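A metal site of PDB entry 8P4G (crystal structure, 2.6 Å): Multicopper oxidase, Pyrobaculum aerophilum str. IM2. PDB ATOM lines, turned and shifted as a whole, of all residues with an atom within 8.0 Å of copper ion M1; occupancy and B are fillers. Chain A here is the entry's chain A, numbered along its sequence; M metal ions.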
ATOM      1  N   HIS A  55      21.217  -4.903   8.923  1.00  0.00           N
ATOM      2  CA  HIS A  55      22.604  -4.530   8.755  1.00  0.00           C
ATOM      3  C   HIS A  55      23.055  -3.743   9.970  1.00  0.00           C
ATOM      4  O   HIS A  55      22.433  -2.743  10.328  1.00  0.00           O
ATOM      5  CB  HIS A  55      22.820  -3.708   7.483  1.00  0.00           C
ATOM      6  CG  HIS A  55      24.195  -3.135   7.381  1.00  0.00           C
ATOM      7  ND1 HIS A  55      25.337  -3.846   7.703  1.00  0.00           N
ATOM      8  CD2 HIS A  55      24.623  -1.893   7.026  1.00  0.00           C
ATOM      9  CE1 HIS A  55      26.393  -3.086   7.530  1.00  0.00           C
ATOM     10  NE2 HIS A  55      25.986  -1.888   7.121  1.00  0.00           N
ATOM     11  N   TRP A  56      24.130  -4.201  10.608  1.00  0.00           N
ATOM     12  CA  TRP A  56      24.748  -3.470  11.714  1.00  0.00           C
ATOM     13  C   TRP A  56      25.714  -2.470  11.096  1.00  0.00           C
ATOM     14  O   TRP A  56      26.875  -2.776  10.833  1.00  0.00           O
ATOM     15  CB  TRP A  56      25.461  -4.425  12.668  1.00  0.00           C
ATOM     16  CG  TRP A  56      24.542  -5.425  13.310  1.00  0.00           C
ATOM     17  CD1 TRP A  56      24.207  -6.654  12.829  1.00  0.00           C
ATOM     18  CD2 TRP A  56      23.857  -5.280  14.553  1.00  0.00           C
ATOM     19  NE1 TRP A  56      23.342  -7.291  13.694  1.00  0.00           N
ATOM     20  CE2 TRP A  56      23.121  -6.457  14.763  1.00  0.00           C
ATOM     21  CE3 TRP A  56      23.795  -4.264  15.517  1.00  0.00           C
ATOM     22  CZ2 TRP A  56      22.322  -6.655  15.899  1.00  0.00           C
ATOM     23  CZ3 TRP A  56      23.002  -4.465  16.637  1.00  0.00           C
ATOM     24  CH2 TRP A  56      22.277  -5.648  16.815  1.00  0.00           C
ATOM     25  N   HIS A  57      25.216  -1.259  10.845  1.00  0.00           N
ATOM     26  CA  HIS A  57      25.960  -0.267  10.096  1.00  0.00           C
ATOM     27  C   HIS A  57      27.254   0.093  10.801  1.00  0.00           C
ATOM     28  O   HIS A  57      27.235   0.610  11.933  1.00  0.00           O
ATOM     29  CB  HIS A  57      25.098   0.976   9.878  1.00  0.00           C
ATOM     30  CG  HIS A  57      25.743   2.025   9.032  1.00  0.00           C
ATOM     31  ND1 HIS A  57      25.249   2.378   7.792  1.00  0.00           N
ATOM     32  CD2 HIS A  57      26.838   2.794   9.228  1.00  0.00           C
ATOM     33  CE1 HIS A  57      26.014   3.330   7.270  1.00  0.00           C
ATOM     34  NE2 HIS A  57      26.985   3.594   8.122  1.00  0.00           N
ATOM     35  N   GLY A  58      28.381  -0.174  10.151  1.00  0.00           N
ATOM     36  CA  GLY A  58      29.689   0.187  10.680  1.00  0.00           C
ATOM     37  C   GLY A  58      30.330  -0.828  11.600  1.00  0.00           C
ATOM     38  O   GLY A  58      31.368  -0.500  12.203  1.00  0.00           O
ATOM     39  N   ASP A  66      26.934  -9.383   8.984  1.00  0.00           N
ATOM     40  CA  ASP A  66      26.918  -8.003   8.482  1.00  0.00           C
ATOM     41  C   ASP A  66      25.518  -7.395   8.508  1.00  0.00           C
ATOM     42  O   ASP A  66      25.332  -6.294   9.055  1.00  0.00           O
ATOM     43  CB  ASP A  66      27.540  -7.952   7.081  1.00  0.00           C
ATOM     44  CG  ASP A  66      27.651  -6.529   6.550  1.00  0.00           C
ATOM     45  OD1 ASP A  66      28.363  -5.717   7.165  1.00  0.00           O
ATOM     46  OD2 ASP A  66      27.017  -6.235   5.518  1.00  0.00           O
ATOM     47  N   ALA A  67      24.498  -8.061   7.941  1.00  0.00           N
ATOM     48  CA  ALA A  67      24.561  -9.298   7.172  1.00  0.00           C
ATOM     49  C   ALA A  67      24.445  -8.997   5.682  1.00  0.00           C
ATOM     50  O   ALA A  67      23.753  -8.060   5.295  1.00  0.00           O
ATOM     51  CB  ALA A  67      23.464 -10.259   7.616  1.00  0.00           C
ATOM     52  N   PRO A  69      23.261  -8.795   2.001  1.00  0.00           N
ATOM     53  CA  PRO A  69      21.861  -8.793   1.547  1.00  0.00           C
ATOM     54  C   PRO A  69      21.391 -10.130   0.992  1.00  0.00           C
ATOM     55  O   PRO A  69      20.188 -10.396   0.997  1.00  0.00           O
ATOM     56  CB  PRO A  69      21.848  -7.709   0.456  1.00  0.00           C
ATOM     57  CG  PRO A  69      22.976  -6.806   0.809  1.00  0.00           C
ATOM     58  CD  PRO A  69      24.037  -7.691   1.406  1.00  0.00           C
ATOM     59  N   HIS A  95      19.546  -1.174  10.547  1.00  0.00           N
ATOM     60  CA  HIS A  95      18.502  -0.840   9.604  1.00  0.00           C
ATOM     61  C   HIS A  95      18.401  -1.955   8.579  1.00  0.00           C
ATOM     62  O   HIS A  95      19.288  -2.821   8.501  1.00  0.00           O
ATOM     63  CB  HIS A  95      18.771   0.513   8.933  1.00  0.00           C
ATOM     64  CG  HIS A  95      20.018   0.550   8.110  1.00  0.00           C
ATOM     65  ND1 HIS A  95      20.110  -0.043   6.870  1.00  0.00           N
ATOM     66  CD2 HIS A  95      21.224   1.136   8.337  1.00  0.00           C
ATOM     67  CE1 HIS A  95      21.324   0.150   6.376  1.00  0.00           C
ATOM     68  NE2 HIS A  95      22.011   0.865   7.242  1.00  0.00           N
ATOM     69  N   PRO A  96      17.333  -1.997   7.782  1.00  0.00           N
ATOM     70  CA  PRO A  96      17.187  -3.095   6.817  1.00  0.00           C
ATOM     71  C   PRO A  96      18.223  -3.009   5.714  1.00  0.00           C
ATOM     72  O   PRO A  96      18.819  -1.964   5.450  1.00  0.00           O
ATOM     73  CB  PRO A  96      15.770  -2.891   6.259  1.00  0.00           C
ATOM     74  CG  PRO A  96      15.089  -1.989   7.200  1.00  0.00           C
ATOM     75  CD  PRO A  96      16.151  -1.112   7.764  1.00  0.00           C
ATOM     76  N   HIS A  97      18.419  -4.146   5.052  1.00  0.00           N
ATOM     77  CA  HIS A  97      19.278  -4.148   3.874  1.00  0.00           C
ATOM     78  C   HIS A  97      18.895  -5.157   2.799  1.00  0.00           C
ATOM     79  O   HIS A  97      19.791  -5.739   2.181  1.00  0.00           O
ATOM     80  CB  HIS A  97      20.722  -4.397   4.307  1.00  0.00           C
ATOM     81  CG  HIS A  97      21.742  -3.639   3.508  1.00  0.00           C
ATOM     82  ND1 HIS A  97      21.966  -3.896   2.176  1.00  0.00           N
ATOM     83  CD2 HIS A  97      22.576  -2.637   3.847  1.00  0.00           C
ATOM     84  CE1 HIS A  97      22.904  -3.081   1.725  1.00  0.00           C
ATOM     85  NE2 HIS A  97      23.295  -2.297   2.718  1.00  0.00           N
ATOM     86  N   THR A 102      15.063  -1.721   0.552  1.00  0.00           N
ATOM     87  CA  THR A 102      15.596  -1.118   1.768  1.00  0.00           C
ATOM     88  C   THR A 102      15.000   0.253   2.026  1.00  0.00           C
ATOM     89  O   THR A 102      14.663   0.577   3.174  1.00  0.00           O
ATOM     90  CB  THR A 102      17.124  -1.028   1.666  1.00  0.00           C
ATOM     91  OG1 THR A 102      17.687  -2.343   1.591  1.00  0.00           O
ATOM     92  CG2 THR A 102      17.696  -0.303   2.868  1.00  0.00           C
ATOM     93  N   ALA A 232      23.200   8.581   7.004  1.00  0.00           N
ATOM     94  CA  ALA A 232      23.905   7.562   7.779  1.00  0.00           C
ATOM     95  C   ALA A 232      25.214   8.055   8.386  1.00  0.00           C
ATOM     96  O   ALA A 232      25.914   7.255   9.026  1.00  0.00           O
ATOM     97  CB  ALA A 232      24.186   6.285   6.974  1.00  0.00           C
ATOM     98  N   HIS A 357      29.397   4.397   1.282  1.00  0.00           N
ATOM     99  CA  HIS A 357      29.599   3.662   2.525  1.00  0.00           C
ATOM    100  C   HIS A 357      30.106   2.261   2.208  1.00  0.00           C
ATOM    101  O   HIS A 357      29.603   1.603   1.294  1.00  0.00           O
ATOM    102  CB  HIS A 357      28.296   3.584   3.334  1.00  0.00           C
ATOM    103  CG  HIS A 357      28.374   2.664   4.508  1.00  0.00           C
ATOM    104  ND1 HIS A 357      29.424   2.657   5.388  1.00  0.00           N
ATOM    105  CD2 HIS A 357      27.520   1.696   4.931  1.00  0.00           C
ATOM    106  CE1 HIS A 357      29.218   1.740   6.317  1.00  0.00           C
ATOM    107  NE2 HIS A 357      28.065   1.142   6.057  1.00  0.00           N
ATOM    108  N   LEU A 358      31.100   1.823   2.969  1.00  0.00           N
ATOM    109  CA  LEU A 358      31.734   0.525   2.774  1.00  0.00           C
ATOM    110  C   LEU A 358      31.529  -0.347   4.009  1.00  0.00           C
ATOM    111  O   LEU A 358      31.829   0.069   5.133  1.00  0.00           O
ATOM    112  CB  LEU A 358      33.238   0.689   2.506  1.00  0.00           C
ATOM    113  CG  LEU A 358      34.086  -0.580   2.411  1.00  0.00           C
ATOM    114  CD1 LEU A 358      33.671  -1.419   1.212  1.00  0.00           C
ATOM    115  CD2 LEU A 358      35.563  -0.226   2.342  1.00  0.00           C
ATOM    116  N   HIS A 359      31.007  -1.554   3.792  1.00  0.00           N
ATOM    117  CA  HIS A 359      30.777  -2.510   4.863  1.00  0.00           C
ATOM    118  C   HIS A 359      32.091  -3.158   5.318  1.00  0.00           C
ATOM    119  O   HIS A 359      33.081  -3.225   4.581  1.00  0.00           O
ATOM    120  CB  HIS A 359      29.811  -3.616   4.426  1.00  0.00           C
ATOM    121  CG  HIS A 359      28.413  -3.145   4.195  1.00  0.00           C
ATOM    122  ND1 HIS A 359      27.311  -3.887   4.579  1.00  0.00           N
ATOM    123  CD2 HIS A 359      27.934  -2.030   3.600  1.00  0.00           C
ATOM    124  CE1 HIS A 359      26.217  -3.235   4.242  1.00  0.00           C
ATOM    125  NE2 HIS A 359      26.556  -2.109   3.644  1.00  0.00           N
ATOM    126  N   THR A 395      31.148   6.341   6.349  1.00  0.00           N
ATOM    127  CA  THR A 395      30.276   6.946   5.347  1.00  0.00           C
ATOM    128  C   THR A 395      30.787   8.352   5.069  1.00  0.00           C
ATOM    129  O   THR A 395      30.733   9.215   5.951  1.00  0.00           O
ATOM    130  CB  THR A 395      28.818   6.982   5.816  1.00  0.00           C
ATOM    131  OG1 THR A 395      28.405   5.665   6.190  1.00  0.00           O
ATOM    132  CG2 THR A 395      27.915   7.507   4.705  1.00  0.00           C
ATOM    133  N   PRO A 420      29.310  -5.251   0.813  1.00  0.00           N
ATOM    134  CA  PRO A 420      28.780  -4.247  -0.119  1.00  0.00           C
ATOM    135  C   PRO A 420      29.499  -2.916   0.018  1.00  0.00           C
ATOM    136  O   PRO A 420      29.932  -2.510   1.100  1.00  0.00           O
ATOM    137  CB  PRO A 420      27.309  -4.129   0.298  1.00  0.00           C
ATOM    138  CG  PRO A 420      27.011  -5.409   1.015  1.00  0.00           C
ATOM    139  CD  PRO A 420      28.281  -5.765   1.720  1.00  0.00           C
ATOM    140  N   PHE A 421      29.627  -2.238  -1.117  1.00  0.00           N
ATOM    141  CA  PHE A 421      30.122  -0.865  -1.190  1.00  0.00           C
ATOM    142  C   PHE A 421      29.126  -0.092  -2.042  1.00  0.00           C
ATOM    143  O   PHE A 421      29.022  -0.312  -3.247  1.00  0.00           O
ATOM    144  CB  PHE A 421      31.525  -0.798  -1.784  1.00  0.00           C
ATOM    145  CG  PHE A 421      32.030   0.603  -1.977  1.00  0.00           C
ATOM    146  CD1 PHE A 421      32.161   1.468  -0.907  1.00  0.00           C
ATOM    147  CD2 PHE A 421      32.402   1.052  -3.236  1.00  0.00           C
ATOM    148  CE1 PHE A 421      32.627   2.761  -1.089  1.00  0.00           C
ATOM    149  CE2 PHE A 421      32.876   2.336  -3.426  1.00  0.00           C
ATOM    150  CZ  PHE A 421      32.990   3.196  -2.343  1.00  0.00           C
ATOM    151  N   HIS A 422      28.382   0.812  -1.406  1.00  0.00           N
ATOM    152  CA  HIS A 422      27.234   1.431  -2.050  1.00  0.00           C
ATOM    153  C   HIS A 422      27.093   2.867  -1.572  1.00  0.00           C
ATOM    154  O   HIS A 422      27.708   3.278  -0.585  1.00  0.00           O
ATOM    155  CB  HIS A 422      25.959   0.652  -1.768  1.00  0.00           C
ATOM    156  CG  HIS A 422      25.579   0.623  -0.318  1.00  0.00           C
ATOM    157  ND1 HIS A 422      24.825   1.613   0.280  1.00  0.00           N
ATOM    158  CD2 HIS A 422      25.863  -0.282   0.661  1.00  0.00           C
ATOM    159  CE1 HIS A 422      24.655   1.321   1.555  1.00  0.00           C
ATOM    160  NE2 HIS A 422      25.268   0.182   1.812  1.00  0.00           N
ATOM    161  N   CYS A 423      26.268   3.617  -2.288  1.00  0.00           N
ATOM    162  CA  CYS A 423      25.859   4.940  -1.839  1.00  0.00           C
ATOM    163  C   CYS A 423      24.720   4.799  -0.845  1.00  0.00           C
ATOM    164  O   CYS A 423      23.828   3.956  -1.021  1.00  0.00           O
ATOM    165  CB  CYS A 423      25.435   5.798  -3.024  1.00  0.00           C
ATOM    166  SG  CYS A 423      24.760   7.392  -2.566  1.00  0.00           S
ATOM    167  N   HIS A 424      24.743   5.612   0.206  1.00  0.00           N
ATOM    168  CA  HIS A 424      23.719   5.520   1.240  1.00  0.00           C
ATOM    169  C   HIS A 424      22.528   6.418   0.961  1.00  0.00           C
ATOM    170  O   HIS A 424      21.655   6.566   1.821  1.00  0.00           O
ATOM    171  CB  HIS A 424      24.315   5.833   2.612  1.00  0.00           C
ATOM    172  CG  HIS A 424      23.897   4.867   3.677  1.00  0.00           C
ATOM    173  ND1 HIS A 424      22.632   4.838   4.211  1.00  0.00           N
ATOM    174  CD2 HIS A 424      24.589   3.881   4.292  1.00  0.00           C
ATOM    175  CE1 HIS A 424      22.552   3.871   5.109  1.00  0.00           C
ATOM    176  NE2 HIS A 424      23.729   3.278   5.178  1.00  0.00           N
ATOM    177  N   LEU A 426      19.318   6.087  -0.264  1.00  0.00           N
ATOM    178  CA  LEU A 426      18.589   4.820  -0.329  1.00  0.00           C
ATOM    179  C   LEU A 426      17.871   4.633  -1.656  1.00  0.00           C
ATOM    180  O   LEU A 426      17.653   3.498  -2.092  1.00  0.00           O
ATOM    181  CB  LEU A 426      17.613   4.728   0.841  1.00  0.00           C
ATOM    182  CG  LEU A 426      18.306   4.746   2.196  1.00  0.00           C
ATOM    183  CD1 LEU A 426      17.321   4.446   3.300  1.00  0.00           C
ATOM    184  CD2 LEU A 426      19.468   3.753   2.219  1.00  0.00           C
ATOM    185  N   GLU A 429      20.737   3.332  -3.811  1.00  0.00           N
ATOM    186  CA  GLU A 429      21.073   1.958  -3.466  1.00  0.00           C
ATOM    187  C   GLU A 429      20.019   0.980  -3.966  1.00  0.00           C
ATOM    188  O   GLU A 429      20.344  -0.047  -4.574  1.00  0.00           O
ATOM    189  CB  GLU A 429      21.247   1.815  -1.958  1.00  0.00           C
ATOM    190  CG  GLU A 429      21.635   0.409  -1.538  1.00  0.00           C
ATOM    191  CD  GLU A 429      21.404   0.159  -0.068  1.00  0.00           C
ATOM    192  OE1 GLU A 429      21.532   1.121   0.721  1.00  0.00           O
ATOM    193  OE2 GLU A 429      21.093  -0.989   0.296  1.00  0.00           O
ATOM    194  N   MET A 434      25.274  -0.331  -5.953  1.00  0.00           N
ATOM    195  CA  MET A 434      25.854  -1.182  -4.917  1.00  0.00           C
ATOM    196  C   MET A 434      26.663  -2.275  -5.614  1.00  0.00           C
ATOM    197  O   MET A 434      26.222  -2.845  -6.607  1.00  0.00           O
ATOM    198  CB  MET A 434      24.777  -1.796  -4.028  1.00  0.00           C
ATOM    199  CG  MET A 434      25.306  -2.735  -2.952  1.00  0.00           C
ATOM    200  SD  MET A 434      24.079  -3.142  -1.706  1.00  0.00           S
ATOM    201  CE  MET A 434      22.897  -4.088  -2.671  1.00  0.00           C
HETATM  202 CU    CU M   1      24.931  -0.749   3.626  1.00  0.00          CU
HETATM  203 CU    CU M   2      27.059  -0.084   6.231  1.00  0.00          CU
HETATM  204 CU    CU M   3      23.737   1.854   6.747  1.00  0.00          CU
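N of His 357 is in hydrogen-bond range of O of His 422 (2.8 Å). ND1 of His 422 sits close to OE1 of Glu 429 (3.4 Å). A ring nitrogen (NE2) of His 55 lies close to a ring nitrogen (ND1) of His 359 (3.5 Å). The backbone carbonyl oxygen of Pro 420 lies within hydrogen-bond range of the backbone NH of His 359 (3.1 Å). The side-chain carboxylate (OD2) of Asp 66 lies within hydrogen-bond range of a ring nitrogen (ND1) of His 359, 2.5 Å away. N of His 55 is in hydrogen-bond range of O of His 95 (2.9 Å). A ring nitrogen (NE2) of His 57 lies close to a ring nitrogen (NE2) of His 357 (3.4 Å). A ring nitrogen (ND1) of His 357 lies within hydrogen-bond range of the side-chain hydroxyl of Thr 395.
Copper ion M1 is bound by a ring nitrogen (NE2) of His 422 (2.1 Å), a ring nitrogen (NE2) of His 359 (2.1 Å) and a ring nitrogen (NE2) of His 97 (2.4 Å). Copper ion M1 has three donor atoms within binding distance.
His 55 touches copper ion M1. CD2 of His 357 touches copper ion M1, at 3.8 Å. Of the 24 residues printed, 5 come within 4 Å of copper ion M1. Along chain A the residues within 4 Å of copper ion M1 span positions 55 to 422.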
